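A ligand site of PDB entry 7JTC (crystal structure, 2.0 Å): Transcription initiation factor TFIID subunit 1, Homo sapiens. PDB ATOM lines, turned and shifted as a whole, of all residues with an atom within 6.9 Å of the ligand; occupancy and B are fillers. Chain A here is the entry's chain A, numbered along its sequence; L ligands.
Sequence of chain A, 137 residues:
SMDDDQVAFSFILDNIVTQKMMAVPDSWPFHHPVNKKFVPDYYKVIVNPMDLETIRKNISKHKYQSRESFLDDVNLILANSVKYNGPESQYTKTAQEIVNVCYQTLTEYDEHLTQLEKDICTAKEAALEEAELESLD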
ATOM      1  N   TRP A  28      24.377   3.246  14.578  1.00  0.00           N
ATOM      2  CA  TRP A  28      23.342   3.108  13.547  1.00  0.00           C
ATOM      3  C   TRP A  28      23.595   3.881  12.244  1.00  0.00           C
ATOM      4  O   TRP A  28      23.224   3.369  11.184  1.00  0.00           O
ATOM      5  CB  TRP A  28      21.955   3.490  14.118  1.00  0.00           C
ATOM      6  CG  TRP A  28      21.875   4.916  14.619  1.00  0.00           C
ATOM      7  CD1 TRP A  28      22.136   5.363  15.892  1.00  0.00           C
ATOM      8  CD2 TRP A  28      21.547   6.082  13.848  1.00  0.00           C
ATOM      9  NE1 TRP A  28      21.979   6.730  15.956  1.00  0.00           N
ATOM     10  CE2 TRP A  28      21.629   7.193  14.723  1.00  0.00           C
ATOM     11  CE3 TRP A  28      21.197   6.295  12.506  1.00  0.00           C
ATOM     12  CZ2 TRP A  28      21.379   8.495  14.298  1.00  0.00           C
ATOM     13  CZ3 TRP A  28      20.947   7.606  12.084  1.00  0.00           C
ATOM     14  CH2 TRP A  28      21.041   8.681  12.978  1.00  0.00           C
ATOM     15  N   PRO A  29      24.190   5.082  12.222  1.00  0.00           N
ATOM     16  CA  PRO A  29      24.321   5.772  10.932  1.00  0.00           C
ATOM     17  C   PRO A  29      25.222   5.028   9.967  1.00  0.00           C
ATOM     18  O   PRO A  29      25.144   5.281   8.753  1.00  0.00           O
ATOM     19  CB  PRO A  29      24.916   7.136  11.293  1.00  0.00           C
ATOM     20  CG  PRO A  29      24.697   7.300  12.784  1.00  0.00           C
ATOM     21  CD  PRO A  29      24.754   5.904  13.323  1.00  0.00           C
ATOM     22  N   PHE A  30      26.074   4.134  10.457  1.00  0.00           N
ATOM     23  CA  PHE A  30      27.035   3.419   9.620  1.00  0.00           C
ATOM     24  C   PHE A  30      26.658   1.974   9.364  1.00  0.00           C
ATOM     25  O   PHE A  30      27.429   1.249   8.717  1.00  0.00           O
ATOM     26  CB  PHE A  30      28.420   3.520  10.255  1.00  0.00           C
ATOM     27  CG  PHE A  30      28.790   4.914  10.654  1.00  0.00           C
ATOM     28  CD1 PHE A  30      29.227   5.836   9.705  1.00  0.00           C
ATOM     29  CD2 PHE A  30      28.680   5.336  11.984  1.00  0.00           C
ATOM     30  CE1 PHE A  30      29.566   7.135  10.069  1.00  0.00           C
ATOM     31  CE2 PHE A  30      29.022   6.642  12.360  1.00  0.00           C
ATOM     32  CZ  PHE A  30      29.457   7.548  11.396  1.00  0.00           C
ATOM     33  N   HIS A  31      25.470   1.536   9.821  1.00  0.00           N
ATOM     34  CA  HIS A  31      25.070   0.141   9.642  1.00  0.00           C
ATOM     35  C   HIS A  31      24.664  -0.206   8.209  1.00  0.00           C
ATOM     36  O   HIS A  31      24.820  -1.360   7.793  1.00  0.00           O
ATOM     37  CB  HIS A  31      23.914  -0.208  10.606  1.00  0.00           C
ATOM     38  CG  HIS A  31      24.367  -0.319  12.012  1.00  0.00           C
ATOM     39  ND1 HIS A  31      23.593  -0.867  13.010  1.00  0.00           N
ATOM     40  CD2 HIS A  31      25.532   0.031  12.608  1.00  0.00           C
ATOM     41  CE1 HIS A  31      24.256  -0.842  14.153  1.00  0.00           C
ATOM     42  NE2 HIS A  31      25.435  -0.285  13.939  1.00  0.00           N
ATOM     43  N   HIS A  32      24.133   0.743   7.435  1.00  0.00           N
ATOM     44  CA  HIS A  32      23.526   0.474   6.131  1.00  0.00           C
ATOM     45  C   HIS A  32      23.843   1.622   5.210  1.00  0.00           C
ATOM     46  O   HIS A  32      24.201   2.718   5.668  1.00  0.00           O
ATOM     47  CB  HIS A  32      21.988   0.346   6.197  1.00  0.00           C
ATOM     48  CG  HIS A  32      21.480  -0.512   7.310  1.00  0.00           C
ATOM     49  ND1 HIS A  32      21.515  -1.889   7.258  1.00  0.00           N
ATOM     50  CD2 HIS A  32      20.937  -0.190   8.514  1.00  0.00           C
ATOM     51  CE1 HIS A  32      21.008  -2.374   8.380  1.00  0.00           C
ATOM     52  NE2 HIS A  32      20.658  -1.373   9.159  1.00  0.00           N
ATOM     53  N   PRO A  33      23.686   1.443   3.890  1.00  0.00           N
ATOM     54  CA  PRO A  33      23.878   2.564   2.965  1.00  0.00           C
ATOM     55  C   PRO A  33      22.892   3.683   3.245  1.00  0.00           C
ATOM     56  O   PRO A  33      21.736   3.453   3.635  1.00  0.00           O
ATOM     57  CB  PRO A  33      23.647   1.942   1.581  1.00  0.00           C
ATOM     58  CG  PRO A  33      23.892   0.488   1.769  1.00  0.00           C
ATOM     59  CD  PRO A  33      23.422   0.177   3.165  1.00  0.00           C
ATOM     60  N   VAL A  34      23.352   4.921   3.031  1.00  0.00           N
ATOM     61  CA  VAL A  34      22.467   6.080   3.184  1.00  0.00           C
ATOM     62  C   VAL A  34      21.366   6.040   2.127  1.00  0.00           C
ATOM     63  O   VAL A  34      21.622   5.760   0.944  1.00  0.00           O
ATOM     64  CB  VAL A  34      23.293   7.373   3.065  1.00  0.00           C
ATOM     65  CG1 VAL A  34      22.382   8.579   3.009  1.00  0.00           C
ATOM     66  CG2 VAL A  34      24.261   7.508   4.242  1.00  0.00           C
ATOM     67  N   ASN A  35      20.120   6.293   2.555  1.00  0.00           N
ATOM     68  CA  ASN A  35      18.966   6.338   1.662  1.00  0.00           C
ATOM     69  C   ASN A  35      18.819   7.752   1.118  1.00  0.00           C
ATOM     70  O   ASN A  35      18.570   8.689   1.885  1.00  0.00           O
ATOM     71  CB  ASN A  35      17.691   5.902   2.395  1.00  0.00           C
ATOM     72  CG  ASN A  35      16.457   5.783   1.478  1.00  0.00           C
ATOM     73  OD1 ASN A  35      16.432   6.297   0.344  1.00  0.00           O
ATOM     74  ND2 ASN A  35      15.435   5.094   1.971  1.00  0.00           N
ATOM     75  N   LYS A  36      18.935   7.898  -0.199  1.00  0.00           N
ATOM     76  CA  LYS A  36      18.855   9.207  -0.840  1.00  0.00           C
ATOM     77  C   LYS A  36      17.541   9.930  -0.505  1.00  0.00           C
ATOM     78  O   LYS A  36      17.498  11.165  -0.508  1.00  0.00           O
ATOM     79  CB  LYS A  36      19.011   9.048  -2.360  1.00  0.00           C
ATOM     80  CG  LYS A  36      19.066  10.332  -3.147  1.00  0.00           C
ATOM     81  CD  LYS A  36      20.032  10.225  -4.334  1.00  0.00           C
ATOM     82  CE  LYS A  36      20.121   8.808  -4.902  1.00  0.00           C
ATOM     83  NZ  LYS A  36      21.400   8.550  -5.641  1.00  0.00           N
ATOM     84  N   LYS A  37      16.475   9.175  -0.232  1.00  0.00           N
ATOM     85  CA  LYS A  37      15.188   9.802   0.078  1.00  0.00           C
ATOM     86  C   LYS A  37      15.185  10.432   1.466  1.00  0.00           C
ATOM     87  O   LYS A  37      14.387  11.342   1.708  1.00  0.00           O
ATOM     88  CB  LYS A  37      14.065   8.766  -0.030  1.00  0.00           C
ATOM     89  CG  LYS A  37      13.675   8.424  -1.479  1.00  0.00           C
ATOM     90  CD  LYS A  37      12.647   7.295  -1.571  1.00  0.00           C
ATOM     91  CE  LYS A  37      11.926   7.270  -2.912  1.00  0.00           C
ATOM     92  NZ  LYS A  37      10.494   7.704  -2.828  1.00  0.00           N
ATOM     93  N   PHE A  38      16.075  10.008   2.361  1.00  0.00           N
ATOM     94  CA  PHE A  38      16.163  10.562   3.705  1.00  0.00           C
ATOM     95  C   PHE A  38      17.271  11.593   3.862  1.00  0.00           C
ATOM     96  O   PHE A  38      17.094  12.544   4.628  1.00  0.00           O
ATOM     97  CB  PHE A  38      16.363   9.428   4.709  1.00  0.00           C
ATOM     98  CG  PHE A  38      15.200   8.478   4.770  1.00  0.00           C
ATOM     99  CD1 PHE A  38      13.929   8.916   4.420  1.00  0.00           C
ATOM    100  CD2 PHE A  38      15.369   7.159   5.166  1.00  0.00           C
ATOM    101  CE1 PHE A  38      12.831   8.049   4.456  1.00  0.00           C
ATOM    102  CE2 PHE A  38      14.275   6.280   5.209  1.00  0.00           C
ATOM    103  CZ  PHE A  38      13.012   6.730   4.858  1.00  0.00           C
ATOM    104  N   VAL A  39      18.378  11.422   3.155  1.00  0.00           N
ATOM    105  CA  VAL A  39      19.480  12.386   3.143  1.00  0.00           C
ATOM    106  C   VAL A  39      19.730  12.782   1.699  1.00  0.00           C
ATOM    107  O   VAL A  39      20.595  12.180   1.037  1.00  0.00           O
ATOM    108  CB  VAL A  39      20.755  11.803   3.785  1.00  0.00           C
ATOM    109  CG1 VAL A  39      21.770  12.898   4.071  1.00  0.00           C
ATOM    110  CG2 VAL A  39      20.420  11.012   5.026  1.00  0.00           C
ATOM    111  N   TYR A  42      23.439  13.491   0.180  1.00  0.00           N
ATOM    112  CA  TYR A  42      24.557  12.643   0.592  1.00  0.00           C
ATOM    113  C   TYR A  42      25.446  12.271  -0.591  1.00  0.00           C
ATOM    114  O   TYR A  42      26.662  12.454  -0.542  1.00  0.00           O
ATOM    115  CB  TYR A  42      24.046  11.387   1.306  1.00  0.00           C
ATOM    116  CG  TYR A  42      25.203  10.635   1.937  1.00  0.00           C
ATOM    117  CD1 TYR A  42      25.773  11.093   3.117  1.00  0.00           C
ATOM    118  CD2 TYR A  42      25.752   9.526   1.318  1.00  0.00           C
ATOM    119  CE1 TYR A  42      26.854  10.436   3.691  1.00  0.00           C
ATOM    120  CE2 TYR A  42      26.857   8.851   1.890  1.00  0.00           C
ATOM    121  CZ  TYR A  42      27.391   9.319   3.064  1.00  0.00           C
ATOM    122  OH  TYR A  42      28.450   8.671   3.639  1.00  0.00           O
ATOM    123  N   ASP A  51      29.661   1.404   4.004  1.00  0.00           N
ATOM    124  CA  ASP A  51      28.903   1.209   5.231  1.00  0.00           C
ATOM    125  C   ASP A  51      29.113  -0.233   5.667  1.00  0.00           C
ATOM    126  O   ASP A  51      29.584  -1.059   4.877  1.00  0.00           O
ATOM    127  CB  ASP A  51      27.432   1.495   4.982  1.00  0.00           C
ATOM    128  CG  ASP A  51      26.852   0.536   3.995  1.00  0.00           C
ATOM    129  OD1 ASP A  51      27.014   0.749   2.778  1.00  0.00           O
ATOM    130  OD2 ASP A  51      26.311  -0.499   4.436  1.00  0.00           O
ATOM    131  N   ASN A  80      34.614   9.227   4.969  1.00  0.00           N
ATOM    132  CA  ASN A  80      33.361   9.798   4.482  1.00  0.00           C
ATOM    133  C   ASN A  80      32.647  10.599   5.578  1.00  0.00           C
ATOM    134  O   ASN A  80      32.043  11.638   5.285  1.00  0.00           O
ATOM    135  CB  ASN A  80      32.439   8.682   3.957  1.00  0.00           C
ATOM    136  CG  ASN A  80      32.927   8.126   2.614  1.00  0.00           C
ATOM    137  OD1 ASN A  80      33.733   8.763   1.935  1.00  0.00           O
ATOM    138  ND2 ASN A  80      32.448   6.950   2.236  1.00  0.00           N
ATOM    139  N   SER A  81      32.687  10.114   6.834  1.00  0.00           N
ATOM    140  CA  SER A  81      32.135  10.901   7.931  1.00  0.00           C
ATOM    141  C   SER A  81      32.889  12.211   8.108  1.00  0.00           C
ATOM    142  O   SER A  81      32.289  13.270   8.336  1.00  0.00           O
ATOM    143  CB  SER A  81      32.166  10.090   9.237  1.00  0.00           C
ATOM    144  OG  SER A  81      31.487  10.769  10.289  1.00  0.00           O
ATOM    145  N   TYR A  84      31.602  14.507   5.132  1.00  0.00           N
ATOM    146  CA  TYR A  84      30.197  14.943   5.173  1.00  0.00           C
ATOM    147  C   TYR A  84      29.836  15.605   6.495  1.00  0.00           C
ATOM    148  O   TYR A  84      29.070  16.580   6.512  1.00  0.00           O
ATOM    149  CB  TYR A  84      29.271  13.751   4.916  1.00  0.00           C
ATOM    150  CG  TYR A  84      27.854  14.211   4.649  1.00  0.00           C
ATOM    151  CD1 TYR A  84      27.460  14.608   3.383  1.00  0.00           C
ATOM    152  CD2 TYR A  84      26.913  14.282   5.674  1.00  0.00           C
ATOM    153  CE1 TYR A  84      26.171  15.048   3.138  1.00  0.00           C
ATOM    154  CE2 TYR A  84      25.618  14.717   5.442  1.00  0.00           C
ATOM    155  CZ  TYR A  84      25.257  15.097   4.169  1.00  0.00           C
ATOM    156  OH  TYR A  84      23.968  15.527   3.922  1.00  0.00           O
ATOM    157  N   ASN A  85      30.345  15.090   7.610  1.00  0.00           N
ATOM    158  CA  ASN A  85      29.947  15.563   8.930  1.00  0.00           C
ATOM    159  C   ASN A  85      30.968  16.478   9.596  1.00  0.00           C
ATOM    160  O   ASN A  85      30.581  17.303  10.443  1.00  0.00           O
ATOM    161  CB  ASN A  85      29.674  14.350   9.829  1.00  0.00           C
ATOM    162  CG  ASN A  85      28.619  13.438   9.221  1.00  0.00           C
ATOM    163  OD1 ASN A  85      27.506  13.887   8.934  1.00  0.00           O
ATOM    164  ND2 ASN A  85      28.971  12.168   8.955  1.00  0.00           N
ATOM    165  N   TYR A  91      29.163  12.302  14.894  1.00  0.00           N
ATOM    166  CA  TYR A  91      29.128  11.178  13.965  1.00  0.00           C
ATOM    167  C   TYR A  91      30.536  10.664  13.682  1.00  0.00           C
ATOM    168  O   TYR A  91      30.761   9.451  13.600  1.00  0.00           O
ATOM    169  CB  TYR A  91      28.439  11.575  12.645  1.00  0.00           C
ATOM    170  CG  TYR A  91      26.928  11.751  12.670  1.00  0.00           C
ATOM    171  CD1 TYR A  91      26.069  10.682  12.914  1.00  0.00           C
ATOM    172  CD2 TYR A  91      26.347  13.000  12.412  1.00  0.00           C
ATOM    173  CE1 TYR A  91      24.696  10.837  12.925  1.00  0.00           C
ATOM    174  CE2 TYR A  91      24.970  13.167  12.416  1.00  0.00           C
ATOM    175  CZ  TYR A  91      24.150  12.085  12.676  1.00  0.00           C
ATOM    176  OH  TYR A  91      22.795  12.244  12.681  1.00  0.00           O
HETATM  177  C1  LIG L   1      24.429  10.769   8.297  1.00  0.00           C
HETATM  178  C2  LIG L   1      25.476   8.684   7.654  1.00  0.00           C
HETATM  179  C3  LIG L   1      20.781   9.084   8.636  1.00  0.00           C
HETATM  180  C4  LIG L   1      20.975   5.599   7.488  1.00  0.00           C
HETATM  181  C5  LIG L   1      21.101   4.207   8.101  1.00  0.00           C
HETATM  182  C6  LIG L   1      22.017   4.606   6.955  1.00  0.00           C
HETATM  183  C7  LIG L   1      21.381   7.027   7.883  1.00  0.00           C
HETATM  184  C8  LIG L   1      22.723   7.424   7.863  1.00  0.00           C
HETATM  185  C9  LIG L   1      22.987   8.730   8.258  1.00  0.00           C
HETATM  186  C10 LIG L   1      24.340  11.275   6.845  1.00  0.00           C
HETATM  187  C11 LIG L   1      25.758  11.207   8.942  1.00  0.00           C
HETATM  188  C12 LIG L   1      26.719   9.107   8.449  1.00  0.00           C
HETATM  189  C13 LIG L   1      20.361  11.701   9.906  1.00  0.00           C
HETATM  190  N1  LIG L   1      18.327   6.750   6.943  1.00  0.00           N
HETATM  191  N2  LIG L   1      24.320   9.310   8.288  1.00  0.00           N
HETATM  192  N3  LIG L   1      22.013   9.543   8.630  1.00  0.00           N
HETATM  193  N4  LIG L   1      20.440   7.869   8.272  1.00  0.00           N
HETATM  194  N5  LIG L   1      19.642   4.662   5.207  1.00  0.00           N
HETATM  195  O1  LIG L   1      26.847  10.494   8.420  1.00  0.00           O
HETATM  196  O2  LIG L   1      19.335   6.616   5.117  1.00  0.00           O
HETATM  197  S1  LIG L   1      19.582   5.761   6.286  1.00  0.00           S
HETATM  198  S2  LIG L   1      19.511  10.252   9.168  1.00  0.00           S
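CZ3 of Trp 28 touches C3 of the ligand (3.8 Å).
O of Pro 29 touches C8 of the ligand, 3.4 Å away.
Phe 30 touches the ligand.
His 32 touches the ligand.
Val 34 touches the ligand.
Phe 38 touches the ligand.
CD1 of Tyr 42 touches C10 of the ligand, 3.998 Å away.
CE2 of Tyr 84 touches C10 of the ligand (3.9 Å).
Tyr 91 touches the ligand.
Hydrophobic or aromatic side chains within 4 Å of the ligand: Trp 28, Pro 29, Phe 30, Val 34, Phe 38, Tyr 42, Tyr 84 and Tyr 91.
Within 4 Å of the ligand: Trp 28, Pro 29, Phe 30, His 32, Pro 33, Val 34, Asn 35, Phe 38, Tyr 42, Tyr 84, Asn 85 and Tyr 91.
The nearest printed residue that does not touch the ligand is Val 39 (4.1 Å).
The backbone carbonyl oxygen (O) of Pro 33 is in hydrogen-bond range of a nitrogen (N5) of the ligand (2.9 Å).
ND2 of Asn 85 sits at hydrogen-bond distance from O1 of the ligand, at 2.8 Å.
The backbone NH (N) of Asn 35 lies within hydrogen-bond range of an oxygen (O2) of the ligand (2.7 Å).
OG of Ser 81 sits at hydrogen-bond distance from ND2 of Asn 85, 3.2 Å away.
The side-chain amide oxygen (OD1) of Asn 35 is in hydrogen-bond range of the backbone NH (N) of Lys 37 (2.9 Å).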
